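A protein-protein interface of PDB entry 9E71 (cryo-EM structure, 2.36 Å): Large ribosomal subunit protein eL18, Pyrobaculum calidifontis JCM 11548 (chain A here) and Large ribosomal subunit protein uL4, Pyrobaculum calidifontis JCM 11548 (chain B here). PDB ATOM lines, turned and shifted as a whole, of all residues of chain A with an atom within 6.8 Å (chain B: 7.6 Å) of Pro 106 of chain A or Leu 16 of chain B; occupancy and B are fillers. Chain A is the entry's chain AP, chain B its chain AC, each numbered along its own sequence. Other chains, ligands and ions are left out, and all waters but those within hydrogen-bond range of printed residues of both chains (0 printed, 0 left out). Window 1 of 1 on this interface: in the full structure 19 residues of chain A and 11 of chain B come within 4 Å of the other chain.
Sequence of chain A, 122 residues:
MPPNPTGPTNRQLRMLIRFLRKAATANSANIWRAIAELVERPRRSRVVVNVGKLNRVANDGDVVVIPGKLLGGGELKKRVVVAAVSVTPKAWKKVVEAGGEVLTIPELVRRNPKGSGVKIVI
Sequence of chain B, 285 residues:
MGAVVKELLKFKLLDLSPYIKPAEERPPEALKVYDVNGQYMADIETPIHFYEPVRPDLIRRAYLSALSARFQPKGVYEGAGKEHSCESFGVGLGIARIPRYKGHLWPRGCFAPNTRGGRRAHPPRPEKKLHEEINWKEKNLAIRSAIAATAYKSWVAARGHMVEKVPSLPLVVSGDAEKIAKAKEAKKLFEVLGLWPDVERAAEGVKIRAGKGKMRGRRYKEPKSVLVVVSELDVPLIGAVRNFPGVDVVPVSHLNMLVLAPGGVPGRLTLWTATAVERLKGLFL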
ATOM      1  N   ARG A  11     -14.485   4.821  32.748  1.00  0.00           N
ATOM      2  CA  ARG A  11     -15.212   3.570  32.582  1.00  0.00           C
ATOM      3  C   ARG A  11     -14.573   2.681  31.528  1.00  0.00           C
ATOM      4  O   ARG A  11     -14.709   1.456  31.597  1.00  0.00           O
ATOM      5  CB  ARG A  11     -16.670   3.853  32.240  1.00  0.00           C
ATOM      6  CG  ARG A  11     -17.563   3.803  33.455  1.00  0.00           C
ATOM      7  CD  ARG A  11     -18.840   4.568  33.248  1.00  0.00           C
ATOM      8  NE  ARG A  11     -19.720   4.449  34.403  1.00  0.00           N
ATOM      9  CZ  ARG A  11     -20.992   4.817  34.411  1.00  0.00           C
ATOM     10  NH1 ARG A  11     -21.568   5.333  33.339  1.00  0.00           N
ATOM     11  NH2 ARG A  11     -21.704   4.662  35.523  1.00  0.00           N
ATOM     12  N   GLN A  12     -13.864   3.267  30.562  1.00  0.00           N
ATOM     13  CA  GLN A  12     -13.104   2.464  29.609  1.00  0.00           C
ATOM     14  C   GLN A  12     -12.025   1.656  30.314  1.00  0.00           C
ATOM     15  O   GLN A  12     -11.874   0.453  30.073  1.00  0.00           O
ATOM     16  CB  GLN A  12     -12.492   3.369  28.544  1.00  0.00           C
ATOM     17  CG  GLN A  12     -13.441   4.428  28.042  1.00  0.00           C
ATOM     18  CD  GLN A  12     -14.676   3.825  27.416  1.00  0.00           C
ATOM     19  OE1 GLN A  12     -15.800   4.214  27.730  1.00  0.00           O
ATOM     20  NE2 GLN A  12     -14.474   2.865  26.524  1.00  0.00           N
ATOM     21  N   ARG A  14     -11.980   0.894  33.532  1.00  0.00           N
ATOM     22  CA  ARG A  14     -12.633  -0.056  34.430  1.00  0.00           C
ATOM     23  C   ARG A  14     -13.093  -1.299  33.676  1.00  0.00           C
ATOM     24  O   ARG A  14     -12.878  -2.434  34.127  1.00  0.00           O
ATOM     25  CB  ARG A  14     -13.810   0.614  35.138  1.00  0.00           C
ATOM     26  CG  ARG A  14     -13.400   1.631  36.183  1.00  0.00           C
ATOM     27  CD  ARG A  14     -14.599   2.189  36.926  1.00  0.00           C
ATOM     28  NE  ARG A  14     -14.937   1.388  38.098  1.00  0.00           N
ATOM     29  CZ  ARG A  14     -14.489   1.619  39.325  1.00  0.00           C
ATOM     30  NH1 ARG A  14     -13.660   2.615  39.582  1.00  0.00           N
ATOM     31  NH2 ARG A  14     -14.879   0.827  40.316  1.00  0.00           N
ATOM     32  N   MET A  15     -13.699  -1.103  32.506  1.00  0.00           N
ATOM     33  CA  MET A  15     -14.135  -2.236  31.702  1.00  0.00           C
ATOM     34  C   MET A  15     -12.951  -3.030  31.175  1.00  0.00           C
ATOM     35  O   MET A  15     -13.025  -4.256  31.068  1.00  0.00           O
ATOM     36  CB  MET A  15     -15.021  -1.751  30.557  1.00  0.00           C
ATOM     37  CG  MET A  15     -16.413  -1.302  30.981  1.00  0.00           C
ATOM     38  SD  MET A  15     -17.450  -2.637  31.608  1.00  0.00           S
ATOM     39  CE  MET A  15     -16.963  -2.690  33.327  1.00  0.00           C
ATOM     40  N   LEU A  16     -11.844  -2.359  30.847  1.00  0.00           N
ATOM     41  CA  LEU A  16     -10.664  -3.082  30.384  1.00  0.00           C
ATOM     42  C   LEU A  16     -10.062  -3.932  31.496  1.00  0.00           C
ATOM     43  O   LEU A  16      -9.612  -5.056  31.249  1.00  0.00           O
ATOM     44  CB  LEU A  16      -9.632  -2.105  29.828  1.00  0.00           C
ATOM     45  CG  LEU A  16      -8.330  -2.728  29.327  1.00  0.00           C
ATOM     46  CD1 LEU A  16      -8.615  -3.843  28.343  1.00  0.00           C
ATOM     47  CD2 LEU A  16      -7.448  -1.672  28.695  1.00  0.00           C
ATOM     48  N   ILE A  17     -10.046  -3.413  32.726  1.00  0.00           N
ATOM     49  CA  ILE A  17      -9.551  -4.193  33.858  1.00  0.00           C
ATOM     50  C   ILE A  17     -10.440  -5.404  34.101  1.00  0.00           C
ATOM     51  O   ILE A  17      -9.950  -6.514  34.357  1.00  0.00           O
ATOM     52  CB  ILE A  17      -9.447  -3.312  35.116  1.00  0.00           C
ATOM     53  CG1 ILE A  17      -8.402  -2.217  34.920  1.00  0.00           C
ATOM     54  CG2 ILE A  17      -9.095  -4.156  36.321  1.00  0.00           C
ATOM     55  CD1 ILE A  17      -8.510  -1.091  35.919  1.00  0.00           C
ATOM     56  N   ARG A  18     -11.762  -5.209  34.033  1.00  0.00           N
ATOM     57  CA  ARG A  18     -12.687  -6.329  34.194  1.00  0.00           C
ATOM     58  C   ARG A  18     -12.497  -7.368  33.095  1.00  0.00           C
ATOM     59  O   ARG A  18     -12.519  -8.578  33.362  1.00  0.00           O
ATOM     60  CB  ARG A  18     -14.127  -5.818  34.205  1.00  0.00           C
ATOM     61  CG  ARG A  18     -15.169  -6.912  34.306  1.00  0.00           C
ATOM     62  CD  ARG A  18     -15.067  -7.633  35.637  1.00  0.00           C
ATOM     63  NE  ARG A  18     -16.038  -8.714  35.744  1.00  0.00           N
ATOM     64  CZ  ARG A  18     -15.881  -9.789  36.503  1.00  0.00           C
ATOM     65  NH1 ARG A  18     -14.807  -9.952  37.256  1.00  0.00           N
ATOM     66  NH2 ARG A  18     -16.825 -10.724  36.506  1.00  0.00           N
ATOM     67  N   PHE A  19     -12.294  -6.909  31.858  1.00  0.00           N
ATOM     68  CA  PHE A  19     -12.045  -7.799  30.731  1.00  0.00           C
ATOM     69  C   PHE A  19     -10.787  -8.622  30.953  1.00  0.00           C
ATOM     70  O   PHE A  19     -10.772  -9.832  30.708  1.00  0.00           O
ATOM     71  CB  PHE A  19     -11.933  -6.964  29.449  1.00  0.00           C
ATOM     72  CG  PHE A  19     -11.435  -7.724  28.246  1.00  0.00           C
ATOM     73  CD1 PHE A  19     -12.304  -8.469  27.477  1.00  0.00           C
ATOM     74  CD2 PHE A  19     -10.107  -7.657  27.858  1.00  0.00           C
ATOM     75  CE1 PHE A  19     -11.854  -9.149  26.371  1.00  0.00           C
ATOM     76  CE2 PHE A  19      -9.657  -8.347  26.758  1.00  0.00           C
ATOM     77  CZ  PHE A  19     -10.531  -9.091  26.014  1.00  0.00           C
ATOM     78  N   LEU A  20      -9.715  -7.975  31.413  1.00  0.00           N
ATOM     79  CA  LEU A  20      -8.457  -8.681  31.619  1.00  0.00           C
ATOM     80  C   LEU A  20      -8.570  -9.705  32.737  1.00  0.00           C
ATOM     81  O   LEU A  20      -8.038 -10.815  32.622  1.00  0.00           O
ATOM     82  CB  LEU A  20      -7.337  -7.687  31.911  1.00  0.00           C
ATOM     83  CG  LEU A  20      -6.795  -6.964  30.682  1.00  0.00           C
ATOM     84  CD1 LEU A  20      -6.004  -5.732  31.080  1.00  0.00           C
ATOM     85  CD2 LEU A  20      -5.949  -7.906  29.853  1.00  0.00           C
ATOM     86  N   ALA A  83       1.062  -4.118  22.052  1.00  0.00           N
ATOM     87  CA  ALA A  83      -0.280  -3.799  22.506  1.00  0.00           C
ATOM     88  C   ALA A  83      -0.175  -2.910  23.734  1.00  0.00           C
ATOM     89  O   ALA A  83       0.726  -3.079  24.556  1.00  0.00           O
ATOM     90  CB  ALA A  83      -1.075  -5.063  22.834  1.00  0.00           C
ATOM     91  N   ALA A  84      -1.081  -1.947  23.846  1.00  0.00           N
ATOM     92  CA  ALA A  84      -0.995  -0.978  24.929  1.00  0.00           C
ATOM     93  C   ALA A  84      -2.387  -0.460  25.249  1.00  0.00           C
ATOM     94  O   ALA A  84      -3.327  -0.616  24.469  1.00  0.00           O
ATOM     95  CB  ALA A  84      -0.057   0.176  24.570  1.00  0.00           C
ATOM     96  N   LEU A 103      -1.561  -2.884  18.452  1.00  0.00           N
ATOM     97  CA  LEU A 103      -2.794  -3.585  18.758  1.00  0.00           C
ATOM     98  C   LEU A 103      -3.355  -3.059  20.067  1.00  0.00           C
ATOM     99  O   LEU A 103      -2.631  -2.511  20.900  1.00  0.00           O
ATOM    100  CB  LEU A 103      -2.574  -5.096  18.891  1.00  0.00           C
ATOM    101  CG  LEU A 103      -2.464  -5.998  17.668  1.00  0.00           C
ATOM    102  CD1 LEU A 103      -1.373  -5.536  16.734  1.00  0.00           C
ATOM    103  CD2 LEU A 103      -2.207  -7.415  18.113  1.00  0.00           C
ATOM    104  N   THR A 104      -4.656  -3.229  20.247  1.00  0.00           N
ATOM    105  CA  THR A 104      -5.233  -3.051  21.565  1.00  0.00           C
ATOM    106  C   THR A 104      -4.973  -4.297  22.395  1.00  0.00           C
ATOM    107  O   THR A 104      -4.738  -5.384  21.860  1.00  0.00           O
ATOM    108  CB  THR A 104      -6.733  -2.780  21.482  1.00  0.00           C
ATOM    109  OG1 THR A 104      -7.421  -3.989  21.144  1.00  0.00           O
ATOM    110  CG2 THR A 104      -7.029  -1.718  20.437  1.00  0.00           C
ATOM    111  N   ILE A 105      -4.985  -4.124  23.718  1.00  0.00           N
ATOM    112  CA  ILE A 105      -4.804  -5.268  24.616  1.00  0.00           C
ATOM    113  C   ILE A 105      -5.891  -6.319  24.440  1.00  0.00           C
ATOM    114  O   ILE A 105      -5.565  -7.513  24.452  1.00  0.00           O
ATOM    115  CB  ILE A 105      -4.661  -4.787  26.066  1.00  0.00           C
ATOM    116  CG1 ILE A 105      -3.325  -4.068  26.253  1.00  0.00           C
ATOM    117  CG2 ILE A 105      -4.757  -5.961  27.022  1.00  0.00           C
ATOM    118  CD1 ILE A 105      -3.188  -3.377  27.583  1.00  0.00           C
ATOM    119  N   PRO A 106      -7.184  -5.977  24.322  1.00  0.00           N
ATOM    120  CA  PRO A 106      -8.175  -7.019  23.995  1.00  0.00           C
ATOM    121  C   PRO A 106      -7.937  -7.702  22.662  1.00  0.00           C
ATOM    122  O   PRO A 106      -8.208  -8.900  22.531  1.00  0.00           O
ATOM    123  CB  PRO A 106      -9.500  -6.250  24.006  1.00  0.00           C
ATOM    124  CG  PRO A 106      -9.268  -5.142  24.920  1.00  0.00           C
ATOM    125  CD  PRO A 106      -7.852  -4.724  24.717  1.00  0.00           C
ATOM    126  N   GLU A 107      -7.443  -6.971  21.665  1.00  0.00           N
ATOM    127  CA  GLU A 107      -7.101  -7.590  20.389  1.00  0.00           C
ATOM    128  C   GLU A 107      -5.963  -8.592  20.576  1.00  0.00           C
ATOM    129  O   GLU A 107      -5.998  -9.696  20.021  1.00  0.00           O
ATOM    130  CB  GLU A 107      -6.742  -6.489  19.380  1.00  0.00           C
ATOM    131  CG  GLU A 107      -5.868  -6.788  18.133  1.00  0.00           C
ATOM    132  CD  GLU A 107      -6.143  -8.092  17.367  1.00  0.00           C
ATOM    133  OE1 GLU A 107      -7.063  -8.861  17.714  1.00  0.00           O
ATOM    134  OE2 GLU A 107      -5.398  -8.356  16.399  1.00  0.00           O
ATOM    135  N   LEU A 108      -4.958  -8.234  21.376  1.00  0.00           N
ATOM    136  CA  LEU A 108      -3.880  -9.174  21.672  1.00  0.00           C
ATOM    137  C   LEU A 108      -4.399 -10.390  22.427  1.00  0.00           C
ATOM    138  O   LEU A 108      -3.958 -11.514  22.177  1.00  0.00           O
ATOM    139  CB  LEU A 108      -2.780  -8.481  22.474  1.00  0.00           C
ATOM    140  CG  LEU A 108      -1.853  -9.369  23.311  1.00  0.00           C
ATOM    141  CD1 LEU A 108      -1.090 -10.356  22.451  1.00  0.00           C
ATOM    142  CD2 LEU A 108      -0.890  -8.531  24.121  1.00  0.00           C
ATOM    143  N   VAL A 109      -5.328 -10.181  23.362  1.00  0.00           N
ATOM    144  CA  VAL A 109      -5.890 -11.291  24.127  1.00  0.00           C
ATOM    145  C   VAL A 109      -6.669 -12.230  23.215  1.00  0.00           C
ATOM    146  O   VAL A 109      -6.601 -13.455  23.354  1.00  0.00           O
ATOM    147  CB  VAL A 109      -6.775 -10.762  25.269  1.00  0.00           C
ATOM    148  CG1 VAL A 109      -7.442 -11.910  25.993  1.00  0.00           C
ATOM    149  CG2 VAL A 109      -5.965  -9.923  26.231  1.00  0.00           C
ATOM    150  N   ARG A 110      -7.431 -11.666  22.275  1.00  0.00           N
ATOM    151  CA  ARG A 110      -8.209 -12.484  21.353  1.00  0.00           C
ATOM    152  C   ARG A 110      -7.308 -13.226  20.377  1.00  0.00           C
ATOM    153  O   ARG A 110      -7.625 -14.344  19.958  1.00  0.00           O
ATOM    154  CB  ARG A 110      -9.210 -11.615  20.595  1.00  0.00           C
ATOM    155  CG  ARG A 110     -10.275 -10.982  21.465  1.00  0.00           C
ATOM    156  CD  ARG A 110     -11.458 -10.528  20.632  1.00  0.00           C
ATOM    157  NE  ARG A 110     -11.180  -9.292  19.910  1.00  0.00           N
ATOM    158  CZ  ARG A 110     -11.465  -8.078  20.362  1.00  0.00           C
ATOM    159  NH1 ARG A 110     -12.025  -7.896  21.546  1.00  0.00           N
ATOM    160  NH2 ARG A 110     -11.181  -7.022  19.606  1.00  0.00           N
ATOM    161  N   ARG A 111      -6.194 -12.611  19.980  1.00  0.00           N
ATOM    162  CA  ARG A 111      -5.274 -13.280  19.067  1.00  0.00           C
ATOM    163  C   ARG A 111      -4.482 -14.371  19.775  1.00  0.00           C
ATOM    164  O   ARG A 111      -4.231 -15.436  19.201  1.00  0.00           O
ATOM    165  CB  ARG A 111      -4.337 -12.257  18.430  1.00  0.00           C
ATOM    166  CG  ARG A 111      -3.174 -12.868  17.684  1.00  0.00           C
ATOM    167  CD  ARG A 111      -2.163 -11.813  17.285  1.00  0.00           C
ATOM    168  NE  ARG A 111      -2.762 -10.776  16.457  1.00  0.00           N
ATOM    169  CZ  ARG A 111      -2.078  -9.841  15.814  1.00  0.00           C
ATOM    170  NH1 ARG A 111      -0.761  -9.775  15.886  1.00  0.00           N
ATOM    171  NH2 ARG A 111      -2.735  -8.947  15.079  1.00  0.00           N
ATOM    172  N   PHE B  11      -8.743   2.295  19.391  1.00  0.00           N
ATOM    173  CA  PHE B  11      -8.690   2.646  20.804  1.00  0.00           C
ATOM    174  C   PHE B  11      -9.888   3.477  21.236  1.00  0.00           C
ATOM    175  O   PHE B  11     -10.219   3.488  22.426  1.00  0.00           O
ATOM    176  CB  PHE B  11      -7.394   3.397  21.113  1.00  0.00           C
ATOM    177  CG  PHE B  11      -6.163   2.543  21.014  1.00  0.00           C
ATOM    178  CD1 PHE B  11      -5.752   1.776  22.086  1.00  0.00           C
ATOM    179  CD2 PHE B  11      -5.425   2.503  19.848  1.00  0.00           C
ATOM    180  CE1 PHE B  11      -4.625   0.987  21.994  1.00  0.00           C
ATOM    181  CE2 PHE B  11      -4.299   1.719  19.753  1.00  0.00           C
ATOM    182  CZ  PHE B  11      -3.901   0.960  20.825  1.00  0.00           C
ATOM    183  N   LEU B  13     -12.996   2.882  20.030  1.00  0.00           N
ATOM    184  CA  LEU B  13     -14.018   1.847  20.144  1.00  0.00           C
ATOM    185  C   LEU B  13     -13.351   0.572  20.658  1.00  0.00           C
ATOM    186  O   LEU B  13     -12.927  -0.291  19.893  1.00  0.00           O
ATOM    187  CB  LEU B  13     -14.753   1.678  18.795  1.00  0.00           C
ATOM    188  CG  LEU B  13     -14.119   1.545  17.394  1.00  0.00           C
ATOM    189  CD1 LEU B  13     -13.432   0.224  17.050  1.00  0.00           C
ATOM    190  CD2 LEU B  13     -15.164   1.884  16.328  1.00  0.00           C
ATOM    191  N   LEU B  14     -13.255   0.456  21.977  1.00  0.00           N
ATOM    192  CA  LEU B  14     -12.566  -0.680  22.571  1.00  0.00           C
ATOM    193  C   LEU B  14     -13.508  -1.875  22.620  1.00  0.00           C
ATOM    194  O   LEU B  14     -14.460  -1.894  23.406  1.00  0.00           O
ATOM    195  CB  LEU B  14     -12.050  -0.329  23.962  1.00  0.00           C
ATOM    196  CG  LEU B  14     -10.971  -1.263  24.509  1.00  0.00           C
ATOM    197  CD1 LEU B  14      -9.720  -1.184  23.654  1.00  0.00           C
ATOM    198  CD2 LEU B  14     -10.649  -0.920  25.953  1.00  0.00           C
ATOM    199  N   ASP B  15     -13.242  -2.866  21.775  1.00  0.00           N
ATOM    200  CA  ASP B  15     -14.047  -4.076  21.703  1.00  0.00           C
ATOM    201  C   ASP B  15     -13.613  -5.032  22.807  1.00  0.00           C
ATOM    202  O   ASP B  15     -12.479  -5.519  22.803  1.00  0.00           O
ATOM    203  CB  ASP B  15     -13.897  -4.729  20.330  1.00  0.00           C
ATOM    204  CG  ASP B  15     -14.924  -5.815  20.081  1.00  0.00           C
ATOM    205  OD1 ASP B  15     -14.885  -6.425  18.994  1.00  0.00           O
ATOM    206  OD2 ASP B  15     -15.770  -6.063  20.964  1.00  0.00           O
ATOM    207  N   LEU B  16     -14.518  -5.306  23.745  1.00  0.00           N
ATOM    208  CA  LEU B  16     -14.222  -6.150  24.891  1.00  0.00           C
ATOM    209  C   LEU B  16     -14.796  -7.554  24.750  1.00  0.00           C
ATOM    210  O   LEU B  16     -14.924  -8.266  25.751  1.00  0.00           O
ATOM    211  CB  LEU B  16     -14.736  -5.500  26.173  1.00  0.00           C
ATOM    212  CG  LEU B  16     -13.973  -4.262  26.645  1.00  0.00           C
ATOM    213  CD1 LEU B  16     -14.481  -3.817  27.998  1.00  0.00           C
ATOM    214  CD2 LEU B  16     -12.481  -4.532  26.692  1.00  0.00           C
ATOM    215  N   SER B  17     -15.155  -7.961  23.539  1.00  0.00           N
ATOM    216  CA  SER B  17     -15.638  -9.314  23.337  1.00  0.00           C
ATOM    217  C   SER B  17     -14.495 -10.311  23.519  1.00  0.00           C
ATOM    218  O   SER B  17     -13.333  -9.991  23.261  1.00  0.00           O
ATOM    219  CB  SER B  17     -16.242  -9.465  21.946  1.00  0.00           C
ATOM    220  OG  SER B  17     -15.293  -9.148  20.944  1.00  0.00           O
ATOM    221  N   PRO B  18     -14.802 -11.537  23.951  1.00  0.00           N
ATOM    222  CA  PRO B  18     -16.129 -12.082  24.245  1.00  0.00           C
ATOM    223  C   PRO B  18     -16.530 -11.991  25.711  1.00  0.00           C
ATOM    224  O   PRO B  18     -17.704 -12.138  26.037  1.00  0.00           O
ATOM    225  CB  PRO B  18     -15.976 -13.540  23.812  1.00  0.00           C
ATOM    226  CG  PRO B  18     -14.561 -13.866  24.211  1.00  0.00           C
ATOM    227  CD  PRO B  18     -13.768 -12.585  24.026  1.00  0.00           C
ATOM    228  N   TYR B  19     -15.583 -11.753  26.621  1.00  0.00           N
ATOM    229  CA  TYR B  19     -15.885 -11.817  28.047  1.00  0.00           C
ATOM    230  C   TYR B  19     -16.762 -10.665  28.523  1.00  0.00           C
ATOM    231  O   TYR B  19     -17.357 -10.765  29.600  1.00  0.00           O
ATOM    232  CB  TYR B  19     -14.591 -11.859  28.857  1.00  0.00           C
ATOM    233  CG  TYR B  19     -13.541 -12.777  28.276  1.00  0.00           C
ATOM    234  CD1 TYR B  19     -12.522 -12.281  27.482  1.00  0.00           C
ATOM    235  CD2 TYR B  19     -13.572 -14.140  28.519  1.00  0.00           C
ATOM    236  CE1 TYR B  19     -11.566 -13.109  26.947  1.00  0.00           C
ATOM    237  CE2 TYR B  19     -12.616 -14.979  27.989  1.00  0.00           C
ATOM    238  CZ  TYR B  19     -11.617 -14.456  27.201  1.00  0.00           C
ATOM    239  OH  TYR B  19     -10.659 -15.282  26.666  1.00  0.00           O
ATOM    240  N   ILE B  20     -16.860  -9.581  27.761  1.00  0.00           N
ATOM    241  CA  ILE B  20     -17.747  -8.471  28.087  1.00  0.00           C
ATOM    242  C   ILE B  20     -18.740  -8.326  26.946  1.00  0.00           C
ATOM    243  O   ILE B  20     -18.343  -8.118  25.795  1.00  0.00           O
ATOM    244  CB  ILE B  20     -16.978  -7.161  28.312  1.00  0.00           C
ATOM    245  CG1 ILE B  20     -16.001  -7.309  29.476  1.00  0.00           C
ATOM    246  CG2 ILE B  20     -17.946  -6.020  28.568  1.00  0.00           C
ATOM    247  CD1 ILE B  20     -16.667  -7.598  30.789  1.00  0.00           C
ATOM    248  N   LYS B  21     -20.021  -8.432  27.262  1.00  0.00           N
ATOM    249  CA  LYS B  21     -21.041  -8.326  26.230  1.00  0.00           C
ATOM    250  C   LYS B  21     -21.142  -6.885  25.743  1.00  0.00           C
ATOM    251  O   LYS B  21     -21.063  -5.958  26.552  1.00  0.00           O
ATOM    252  CB  LYS B  21     -22.392  -8.815  26.751  1.00  0.00           C
ATOM    253  CG  LYS B  21     -22.617 -10.350  26.814  1.00  0.00           C
ATOM    254  CD  LYS B  21     -21.695 -11.281  25.983  1.00  0.00           C
ATOM    255  CE  LYS B  21     -21.593 -10.969  24.484  1.00  0.00           C
ATOM    256  NZ  LYS B  21     -20.410 -11.619  23.858  1.00  0.00           N
ATOM    257  N   PRO B  22     -21.301  -6.658  24.443  1.00  0.00           N
ATOM    258  CA  PRO B  22     -21.292  -5.288  23.926  1.00  0.00           C
ATOM    259  C   PRO B  22     -22.521  -4.505  24.357  1.00  0.00           C
ATOM    260  O   PRO B  22     -23.570  -5.057  24.695  1.00  0.00           O
ATOM    261  CB  PRO B  22     -21.266  -5.481  22.406  1.00  0.00           C
ATOM    262  CG  PRO B  22     -20.813  -6.897  22.204  1.00  0.00           C
ATOM    263  CD  PRO B  22     -21.384  -7.648  23.362  1.00  0.00           C
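N of Glu 107 of chain A sits at hydrogen-bond distance from OG1 of Thr 104 of chain A, 3.0 Å away.
N of Ala 84 of chain A is in hydrogen-bond range of O of Leu 103 of chain A (3.4 Å).
The side-chain carboxylate (OD2) of Asp 15 of chain B lies within hydrogen-bond range of the side-chain hydroxyl (OG) of Ser 17 of chain B, 3.1 Å away.
Of the 11 printed residues of chain B, 6 touch a printed residue of chain A.
Hydrophobic or aromatic side chains of chain B within 4 Å of the printed part of chain A: Phe 11, Leu 16, Tyr 19 and Ile 20.
Hydrophobic or aromatic side chains of chain A within 4 Å of the printed part of chain B: Met 15, Phe 19 and Pro 106.
Along chain A the printed residues that touch a printed residue of chain B span positions 15 to 110.
Among the printed residues, 12 pairs touch across the chains.
Among the printed residues, Asp or Glu carboxylates within 4 Å of a Lys or Arg side-chain nitrogen of the other chain: Arg 110 of chain A with Asp 15 of chain B.
Met 15 of chain A touches Leu 16 of chain B (CB to CD1, 3.3 Å).
Arg 18 of chain A touches Ile 20 of chain B (CG to CD1, 3.9 Å).
CD1 of Phe 19 of chain A touches O of Leu 16 of chain B, at 3.1 Å.
Phe 19 of chain A touches Ser 17 of chain B (CE1 to O, 3.5 Å).
CD1 of Tyr 19 of chain B touches CE1 of Phe 19 of chain A, 3.4 Å away.
O of Ala 84 of chain A touches CE1 of Phe 11 of chain B (3.2 Å).
O of Leu 103 of chain A touches CZ of Phe 11 of chain B, at 3.7 Å.
Thr 104 of chain A touches Phe 11 of chain B.
O of Asp 15 of chain B touches CB of Pro 106 of chain A (3.3 Å).
CD2 of Leu 16 of chain B touches CG of Pro 106 of chain A, at 3.7 Å.
Of the printed residues of chain B, Pro 106 of chain A touches Asp 15 (3.3 Å) and Leu 16 (3.7 Å).
Of chain A, only Met 15 (3.3 Å), Phe 19 (3.1 Å) and Pro 106 (3.7 Å) come within 4 Å of Leu 16 of chain B.
Printed residues of chain A within 4 Å of Tyr 19 of chain B: Phe 19 (3.4 Å).
Printed residues of chain A within 4 Å of Phe 11 of chain B: Ala 84, Leu 103 and Thr 104.
Printed residues of chain B within 4 Å of Met 15 of chain A: Leu 16.
Of the printed residues of chain B, Arg 110 of chain A touches Asp 15 (2.7 Å) and Ser 17 (3.0 Å).
Of the printed residues of chain B, Arg 18 of chain A touches Ile 20.
Arg 14 of chain A touches none of the printed residues of chain B.
The nearest residue of chain A that does not touch Leu 16 of chain B is Leu 16 of chain A (4.1 Å).
The backbone carbonyl oxygen (O) of Ser 17 of chain B sits at hydrogen-bond distance from the guanidinium group (NH1) of Arg 110 of chain A (3.0 Å).
The side-chain carboxylate of Asp 15 of chain B is in salt-bridge range of the guanidinium group of Arg 110 of chain A (3.8 Å).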
